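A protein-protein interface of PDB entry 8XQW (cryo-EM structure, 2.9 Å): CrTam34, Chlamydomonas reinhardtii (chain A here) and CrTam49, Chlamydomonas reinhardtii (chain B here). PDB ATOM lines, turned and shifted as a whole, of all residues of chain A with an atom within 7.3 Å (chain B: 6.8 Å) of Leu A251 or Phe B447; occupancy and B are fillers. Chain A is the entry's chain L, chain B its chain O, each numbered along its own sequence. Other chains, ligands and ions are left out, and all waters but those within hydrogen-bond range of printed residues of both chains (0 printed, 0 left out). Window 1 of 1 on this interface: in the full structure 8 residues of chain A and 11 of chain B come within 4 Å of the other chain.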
ATOM      1  N   HIS A 245      13.727  -8.944 -11.406  1.00  0.00           N
ATOM      2  CA  HIS A 245      12.656  -8.630 -10.484  1.00  0.00           C
ATOM      3  C   HIS A 245      11.956  -9.930 -10.112  1.00  0.00           C
ATOM      4  O   HIS A 245      12.456 -11.021 -10.384  1.00  0.00           O
ATOM      5  CB  HIS A 245      11.705  -7.623 -11.119  1.00  0.00           C
ATOM      6  CG  HIS A 245      11.240  -6.561 -10.180  1.00  0.00           C
ATOM      7  ND1 HIS A 245       9.925  -6.441  -9.786  1.00  0.00           N
ATOM      8  CD2 HIS A 245      11.911  -5.565  -9.561  1.00  0.00           C
ATOM      9  CE1 HIS A 245       9.807  -5.418  -8.962  1.00  0.00           C
ATOM     10  NE2 HIS A 245      10.999  -4.870  -8.807  1.00  0.00           N
ATOM     11  N   LEU A 246      10.797  -9.837  -9.474  1.00  0.00           N
ATOM     12  CA  LEU A 246       9.922 -10.989  -9.335  1.00  0.00           C
ATOM     13  C   LEU A 246       8.672 -10.880 -10.179  1.00  0.00           C
ATOM     14  O   LEU A 246       8.253 -11.874 -10.766  1.00  0.00           O
ATOM     15  CB  LEU A 246       9.515 -11.192  -7.875  1.00  0.00           C
ATOM     16  CG  LEU A 246       8.713 -12.472  -7.623  1.00  0.00           C
ATOM     17  CD1 LEU A 246       9.617 -13.677  -7.594  1.00  0.00           C
ATOM     18  CD2 LEU A 246       7.921 -12.381  -6.342  1.00  0.00           C
ATOM     19  N   VAL A 247       8.076  -9.693 -10.259  1.00  0.00           N
ATOM     20  CA  VAL A 247       6.950  -9.486 -11.157  1.00  0.00           C
ATOM     21  C   VAL A 247       7.328  -9.858 -12.577  1.00  0.00           C
ATOM     22  O   VAL A 247       6.489 -10.327 -13.350  1.00  0.00           O
ATOM     23  CB  VAL A 247       6.476  -8.026 -11.071  1.00  0.00           C
ATOM     24  CG1 VAL A 247       5.232  -7.822 -11.893  1.00  0.00           C
ATOM     25  CG2 VAL A 247       6.227  -7.653  -9.637  1.00  0.00           C
ATOM     26  N   TRP A 248       8.590  -9.676 -12.939  1.00  0.00           N
ATOM     27  CA  TRP A 248       9.028  -9.903 -14.304  1.00  0.00           C
ATOM     28  C   TRP A 248       9.614 -11.284 -14.513  1.00  0.00           C
ATOM     29  O   TRP A 248       9.460 -11.851 -15.595  1.00  0.00           O
ATOM     30  CB  TRP A 248      10.045  -8.835 -14.702  1.00  0.00           C
ATOM     31  CG  TRP A 248       9.436  -7.500 -14.776  1.00  0.00           C
ATOM     32  CD1 TRP A 248       9.628  -6.471 -13.926  1.00  0.00           C
ATOM     33  CD2 TRP A 248       8.496  -7.052 -15.746  1.00  0.00           C
ATOM     34  NE1 TRP A 248       8.870  -5.396 -14.304  1.00  0.00           N
ATOM     35  CE2 TRP A 248       8.165  -5.732 -15.425  1.00  0.00           C
ATOM     36  CE3 TRP A 248       7.906  -7.639 -16.862  1.00  0.00           C
ATOM     37  CZ2 TRP A 248       7.274  -4.992 -16.174  1.00  0.00           C
ATOM     38  CZ3 TRP A 248       7.025  -6.902 -17.604  1.00  0.00           C
ATOM     39  CH2 TRP A 248       6.713  -5.594 -17.259  1.00  0.00           C
ATOM     40  N   ALA A 249      10.263 -11.854 -13.506  1.00  0.00           N
ATOM     41  CA  ALA A 249      10.892 -13.152 -13.692  1.00  0.00           C
ATOM     42  C   ALA A 249       9.905 -14.302 -13.578  1.00  0.00           C
ATOM     43  O   ALA A 249      10.058 -15.302 -14.280  1.00  0.00           O
ATOM     44  CB  ALA A 249      12.022 -13.341 -12.686  1.00  0.00           C
ATOM     45  N   VAL A 250       8.898 -14.197 -12.715  1.00  0.00           N
ATOM     46  CA  VAL A 250       8.023 -15.335 -12.462  1.00  0.00           C
ATOM     47  C   VAL A 250       6.554 -15.005 -12.693  1.00  0.00           C
ATOM     48  O   VAL A 250       5.830 -15.783 -13.317  1.00  0.00           O
ATOM     49  CB  VAL A 250       8.230 -15.868 -11.037  1.00  0.00           C
ATOM     50  CG1 VAL A 250       7.252 -16.970 -10.748  1.00  0.00           C
ATOM     51  CG2 VAL A 250       9.633 -16.379 -10.879  1.00  0.00           C
ATOM     52  N   LEU A 251       6.094 -13.864 -12.188  1.00  0.00           N
ATOM     53  CA  LEU A 251       4.654 -13.630 -12.128  1.00  0.00           C
ATOM     54  C   LEU A 251       4.058 -13.263 -13.479  1.00  0.00           C
ATOM     55  O   LEU A 251       2.973 -13.738 -13.822  1.00  0.00           O
ATOM     56  CB  LEU A 251       4.339 -12.547 -11.102  1.00  0.00           C
ATOM     57  CG  LEU A 251       4.603 -12.942  -9.650  1.00  0.00           C
ATOM     58  CD1 LEU A 251       4.153 -11.857  -8.702  1.00  0.00           C
ATOM     59  CD2 LEU A 251       3.908 -14.242  -9.333  1.00  0.00           C
ATOM     60  N   ALA A 252       4.718 -12.415 -14.250  1.00  0.00           N
ATOM     61  CA  ALA A 252       4.151 -12.016 -15.535  1.00  0.00           C
ATOM     62  C   ALA A 252       4.260 -13.120 -16.581  1.00  0.00           C
ATOM     63  O   ALA A 252       3.335 -13.289 -17.387  1.00  0.00           O
ATOM     64  CB  ALA A 252       4.814 -10.742 -16.048  1.00  0.00           C
ATOM     65  N   PRO A 253       5.366 -13.864 -16.642  1.00  0.00           N
ATOM     66  CA  PRO A 253       5.376 -15.031 -17.523  1.00  0.00           C
ATOM     67  C   PRO A 253       4.276 -16.017 -17.210  1.00  0.00           C
ATOM     68  O   PRO A 253       3.750 -16.644 -18.127  1.00  0.00           O
ATOM     69  CB  PRO A 253       6.757 -15.633 -17.278  1.00  0.00           C
ATOM     70  CG  PRO A 253       7.569 -14.513 -16.919  1.00  0.00           C
ATOM     71  CD  PRO A 253       6.717 -13.584 -16.137  1.00  0.00           C
ATOM     72  N   LEU A 254       3.912 -16.181 -15.942  1.00  0.00           N
ATOM     73  CA  LEU A 254       2.822 -17.089 -15.606  1.00  0.00           C
ATOM     74  C   LEU A 254       1.530 -16.659 -16.281  1.00  0.00           C
ATOM     75  O   LEU A 254       0.847 -17.470 -16.914  1.00  0.00           O
ATOM     76  CB  LEU A 254       2.639 -17.147 -14.096  1.00  0.00           C
ATOM     77  CG  LEU A 254       3.182 -18.395 -13.425  1.00  0.00           C
ATOM     78  CD1 LEU A 254       3.025 -18.288 -11.932  1.00  0.00           C
ATOM     79  CD2 LEU A 254       2.431 -19.571 -13.936  1.00  0.00           C
ATOM     80  N   ALA A 255       1.184 -15.379 -16.165  1.00  0.00           N
ATOM     81  CA  ALA A 255      -0.037 -14.892 -16.789  1.00  0.00           C
ATOM     82  C   ALA A 255       0.025 -15.023 -18.302  1.00  0.00           C
ATOM     83  O   ALA A 255      -0.935 -15.485 -18.931  1.00  0.00           O
ATOM     84  CB  ALA A 255      -0.277 -13.441 -16.395  1.00  0.00           C
ATOM     85  N   LEU A 256       1.142 -14.633 -18.908  1.00  0.00           N
ATOM     86  CA  LEU A 256       1.204 -14.654 -20.363  1.00  0.00           C
ATOM     87  C   LEU A 256       1.207 -16.077 -20.900  1.00  0.00           C
ATOM     88  O   LEU A 256       0.584 -16.356 -21.927  1.00  0.00           O
ATOM     89  CB  LEU A 256       2.424 -13.883 -20.843  1.00  0.00           C
ATOM     90  CG  LEU A 256       2.324 -12.380 -20.603  1.00  0.00           C
ATOM     91  CD1 LEU A 256       3.591 -11.708 -21.044  1.00  0.00           C
ATOM     92  CD2 LEU A 256       1.137 -11.808 -21.330  1.00  0.00           C
ATOM     93  N   LEU A 257       1.879 -16.998 -20.215  1.00  0.00           N
ATOM     94  CA  LEU A 257       1.849 -18.393 -20.630  1.00  0.00           C
ATOM     95  C   LEU A 257       0.462 -18.985 -20.464  1.00  0.00           C
ATOM     96  O   LEU A 257       0.014 -19.763 -21.307  1.00  0.00           O
ATOM     97  CB  LEU A 257       2.855 -19.202 -19.823  1.00  0.00           C
ATOM     98  CG  LEU A 257       4.315 -19.096 -20.220  1.00  0.00           C
ATOM     99  CD1 LEU A 257       5.116 -20.058 -19.402  1.00  0.00           C
ATOM    100  CD2 LEU A 257       4.454 -19.419 -21.665  1.00  0.00           C
ATOM    101  N   LEU A 275      10.224 -22.401 -16.015  1.00  0.00           N
ATOM    102  CA  LEU A 275      10.081 -21.123 -15.331  1.00  0.00           C
ATOM    103  C   LEU A 275      10.798 -21.149 -13.999  1.00  0.00           C
ATOM    104  O   LEU A 275      11.624 -20.282 -13.715  1.00  0.00           O
ATOM    105  CB  LEU A 275       8.612 -20.792 -15.123  1.00  0.00           C
ATOM    106  CG  LEU A 275       7.904 -19.941 -16.163  1.00  0.00           C
ATOM    107  CD1 LEU A 275       6.460 -19.796 -15.778  1.00  0.00           C
ATOM    108  CD2 LEU A 275       8.561 -18.594 -16.264  1.00  0.00           C
ATOM    109  N   VAL B 440      -1.185 -17.931  -2.022  1.00  0.00           N
ATOM    110  CA  VAL B 440      -0.335 -17.666  -3.177  1.00  0.00           C
ATOM    111  C   VAL B 440      -1.167 -17.638  -4.450  1.00  0.00           C
ATOM    112  O   VAL B 440      -0.903 -16.842  -5.357  1.00  0.00           O
ATOM    113  CB  VAL B 440       0.821 -18.679  -3.269  1.00  0.00           C
ATOM    114  CG1 VAL B 440       1.659 -18.636  -2.010  1.00  0.00           C
ATOM    115  CG2 VAL B 440       0.317 -20.074  -3.530  1.00  0.00           C
ATOM    116  N   ARG B 442      -4.236 -16.559  -4.642  1.00  0.00           N
ATOM    117  CA  ARG B 442      -4.907 -15.268  -4.669  1.00  0.00           C
ATOM    118  C   ARG B 442      -3.972 -14.173  -5.158  1.00  0.00           C
ATOM    119  O   ARG B 442      -4.347 -13.369  -6.022  1.00  0.00           O
ATOM    120  CB  ARG B 442      -5.456 -14.932  -3.287  1.00  0.00           C
ATOM    121  CG  ARG B 442      -6.552 -13.880  -3.299  1.00  0.00           C
ATOM    122  CD  ARG B 442      -7.747 -14.325  -4.129  1.00  0.00           C
ATOM    123  NE  ARG B 442      -8.189 -15.673  -3.783  1.00  0.00           N
ATOM    124  CZ  ARG B 442      -8.960 -15.964  -2.740  1.00  0.00           C
ATOM    125  NH1 ARG B 442      -9.315 -17.217  -2.502  1.00  0.00           N
ATOM    126  NH2 ARG B 442      -9.376 -14.999  -1.932  1.00  0.00           N
ATOM    127  N   VAL B 443      -2.748 -14.123  -4.631  1.00  0.00           N
ATOM    128  CA  VAL B 443      -1.851 -13.050  -5.058  1.00  0.00           C
ATOM    129  C   VAL B 443      -1.463 -13.224  -6.523  1.00  0.00           C
ATOM    130  O   VAL B 443      -1.326 -12.242  -7.264  1.00  0.00           O
ATOM    131  CB  VAL B 443      -0.615 -12.951  -4.143  1.00  0.00           C
ATOM    132  CG1 VAL B 443      -1.031 -13.003  -2.692  1.00  0.00           C
ATOM    133  CG2 VAL B 443       0.393 -14.032  -4.452  1.00  0.00           C
ATOM    134  N   ALA B 444      -1.326 -14.467  -6.979  1.00  0.00           N
ATOM    135  CA  ALA B 444      -0.991 -14.692  -8.375  1.00  0.00           C
ATOM    136  C   ALA B 444      -2.150 -14.314  -9.284  1.00  0.00           C
ATOM    137  O   ALA B 444      -1.937 -13.762 -10.365  1.00  0.00           O
ATOM    138  CB  ALA B 444      -0.586 -16.145  -8.590  1.00  0.00           C
ATOM    139  N   CYS B 445      -3.384 -14.597  -8.866  1.00  0.00           N
ATOM    140  CA  CYS B 445      -4.532 -14.177  -9.656  1.00  0.00           C
ATOM    141  C   CYS B 445      -4.601 -12.663  -9.744  1.00  0.00           C
ATOM    142  O   CYS B 445      -4.910 -12.109 -10.806  1.00  0.00           O
ATOM    143  CB  CYS B 445      -5.819 -14.730  -9.059  1.00  0.00           C
ATOM    144  SG  CYS B 445      -7.297 -14.287  -9.983  1.00  0.00           S
ATOM    145  N   TRP B 446      -4.299 -11.974  -8.647  1.00  0.00           N
ATOM    146  CA  TRP B 446      -4.309 -10.518  -8.695  1.00  0.00           C
ATOM    147  C   TRP B 446      -3.254  -9.991  -9.658  1.00  0.00           C
ATOM    148  O   TRP B 446      -3.528  -9.109 -10.479  1.00  0.00           O
ATOM    149  CB  TRP B 446      -4.100  -9.928  -7.309  1.00  0.00           C
ATOM    150  CG  TRP B 446      -4.378  -8.474  -7.311  1.00  0.00           C
ATOM    151  CD1 TRP B 446      -5.599  -7.881  -7.383  1.00  0.00           C
ATOM    152  CD2 TRP B 446      -3.418  -7.416  -7.282  1.00  0.00           C
ATOM    153  NE1 TRP B 446      -5.462  -6.518  -7.386  1.00  0.00           N
ATOM    154  CE2 TRP B 446      -4.129  -6.207  -7.324  1.00  0.00           C
ATOM    155  CE3 TRP B 446      -2.025  -7.374  -7.215  1.00  0.00           C
ATOM    156  CZ2 TRP B 446      -3.499  -4.972  -7.299  1.00  0.00           C
ATOM    157  CZ3 TRP B 446      -1.402  -6.148  -7.192  1.00  0.00           C
ATOM    158  CH2 TRP B 446      -2.137  -4.964  -7.234  1.00  0.00           C
ATOM    159  N   PHE B 447      -2.034 -10.522  -9.581  1.00  0.00           N
ATOM    160  CA  PHE B 447      -0.990 -10.007 -10.459  1.00  0.00           C
ATOM    161  C   PHE B 447      -1.217 -10.404 -11.911  1.00  0.00           C
ATOM    162  O   PHE B 447      -0.809  -9.676 -12.818  1.00  0.00           O
ATOM    163  CB  PHE B 447       0.375 -10.462  -9.974  1.00  0.00           C
ATOM    164  CG  PHE B 447       1.005  -9.501  -9.031  1.00  0.00           C
ATOM    165  CD1 PHE B 447       0.690  -9.527  -7.692  1.00  0.00           C
ATOM    166  CD2 PHE B 447       1.883  -8.544  -9.484  1.00  0.00           C
ATOM    167  CE1 PHE B 447       1.254  -8.632  -6.821  1.00  0.00           C
ATOM    168  CE2 PHE B 447       2.451  -7.646  -8.615  1.00  0.00           C
ATOM    169  CZ  PHE B 447       2.137  -7.691  -7.283  1.00  0.00           C
ATOM    170  N   ALA B 448      -1.880 -11.528 -12.156  1.00  0.00           N
ATOM    171  CA  ALA B 448      -2.296 -11.839 -13.516  1.00  0.00           C
ATOM    172  C   ALA B 448      -3.311 -10.823 -14.018  1.00  0.00           C
ATOM    173  O   ALA B 448      -3.211 -10.345 -15.155  1.00  0.00           O
ATOM    174  CB  ALA B 448      -2.875 -13.247 -13.576  1.00  0.00           C
ATOM    175  N   GLU B 449      -4.301 -10.485 -13.188  1.00  0.00           N
ATOM    176  CA  GLU B 449      -5.261  -9.458 -13.576  1.00  0.00           C
ATOM    177  C   GLU B 449      -4.578  -8.126 -13.815  1.00  0.00           C
ATOM    178  O   GLU B 449      -5.071  -7.308 -14.596  1.00  0.00           O
ATOM    179  CB  GLU B 449      -6.335  -9.295 -12.505  1.00  0.00           C
ATOM    180  CG  GLU B 449      -7.316 -10.445 -12.413  1.00  0.00           C
ATOM    181  CD  GLU B 449      -8.298 -10.271 -11.269  1.00  0.00           C
ATOM    182  OE1 GLU B 449      -8.645  -9.115 -10.954  1.00  0.00           O
ATOM    183  OE2 GLU B 449      -8.715 -11.290 -10.681  1.00  0.00           O
ATOM    184  N   LEU B 450      -3.461  -7.881 -13.140  1.00  0.00           N
ATOM    185  CA  LEU B 450      -2.735  -6.633 -13.345  1.00  0.00           C
ATOM    186  C   LEU B 450      -1.980  -6.629 -14.667  1.00  0.00           C
ATOM    187  O   LEU B 450      -2.071  -5.661 -15.434  1.00  0.00           O
ATOM    188  CB  LEU B 450      -1.766  -6.398 -12.197  1.00  0.00           C
ATOM    189  CG  LEU B 450      -1.043  -5.062 -12.256  1.00  0.00           C
ATOM    190  CD1 LEU B 450      -2.010  -3.956 -11.910  1.00  0.00           C
ATOM    191  CD2 LEU B 450       0.143  -5.051 -11.320  1.00  0.00           C
ATOM    192  N   THR B 451      -1.224  -7.689 -14.949  1.00  0.00           N
ATOM    193  CA  THR B 451      -0.450  -7.704 -16.181  1.00  0.00           C
ATOM    194  C   THR B 451      -1.332  -7.807 -17.409  1.00  0.00           C
ATOM    195  O   THR B 451      -0.947  -7.325 -18.471  1.00  0.00           O
ATOM    196  CB  THR B 451       0.558  -8.842 -16.192  1.00  0.00           C
ATOM    197  OG1 THR B 451      -0.129 -10.075 -16.406  1.00  0.00           O
ATOM    198  CG2 THR B 451       1.326  -8.890 -14.892  1.00  0.00           C
ATOM    199  N   MET B 452      -2.516  -8.407 -17.301  1.00  0.00           N
ATOM    200  CA  MET B 452      -3.406  -8.418 -18.458  1.00  0.00           C
ATOM    201  C   MET B 452      -3.878  -7.012 -18.801  1.00  0.00           C
ATOM    202  O   MET B 452      -3.892  -6.618 -19.973  1.00  0.00           O
ATOM    203  CB  MET B 452      -4.592  -9.334 -18.199  1.00  0.00           C
ATOM    204  CG  MET B 452      -4.244 -10.798 -18.268  1.00  0.00           C
ATOM    205  SD  MET B 452      -4.150 -11.407 -19.951  1.00  0.00           S
ATOM    206  CE  MET B 452      -2.401 -11.702 -20.081  1.00  0.00           C
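O of Ala B448 sits at hydrogen-bond distance from OG1 of Thr B451, at 3.3 Å.
N of Ala A252 lies within hydrogen-bond range of O of Val A247 (2.9 Å).
O of Leu A246 sits at hydrogen-bond distance from N of Leu A251.
Among the printed residues, pairs that only touch across the chains: Ala A255 with Thr B451, Leu A256 with Met B452, Ala A255 with Ala B448, Val A247 with Phe B447 and Leu A251 with Phe B447.
Printed residues of chain B within 4 Å of Leu A251: Phe B447 (3.9 Å).
Of chain A, only Val A247 (3.9 Å) and Leu A251 (3.9 Å) come within 4 Å of Phe B447.
Of the printed residues of chain A, Thr B451 touches Ala A255.
Printed residues of chain B within 4 Å of Ala A255: Ala B448 and Thr B451.
Printed residues of chain B within 4 Å of Val A247: Phe B447 (3.9 Å).
Of the printed residues of chain A, Met B452 touches Leu A256 (3.8 Å).
Of the printed residues of chain A, Ala B448 touches Ala A255 (3.8 Å).
Val B443 touches none of the printed residues of chain A.
The nearest residue of chain B that does not touch Leu A251 is Ala B444 (4.9 Å).
The nearest residue of chain A that does not touch Phe B447 is Ala A255 (5.2 Å).
Of the 12 printed residues of chain B, 4 touch a printed residue of chain A.
Hydrophobic or aromatic side chains of chain B that line the printed part of chain A: Phe B447, Ala B448 and Met B452.
Printed residues of chain A that touch a printed residue of chain B: Val A247, Leu A251, Ala A255 and Leu A256.
Hydrophobic or aromatic side chains of chain A within 4 Å of the printed part of chain B: Val A247, Leu A251, Ala A255 and Leu A256.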
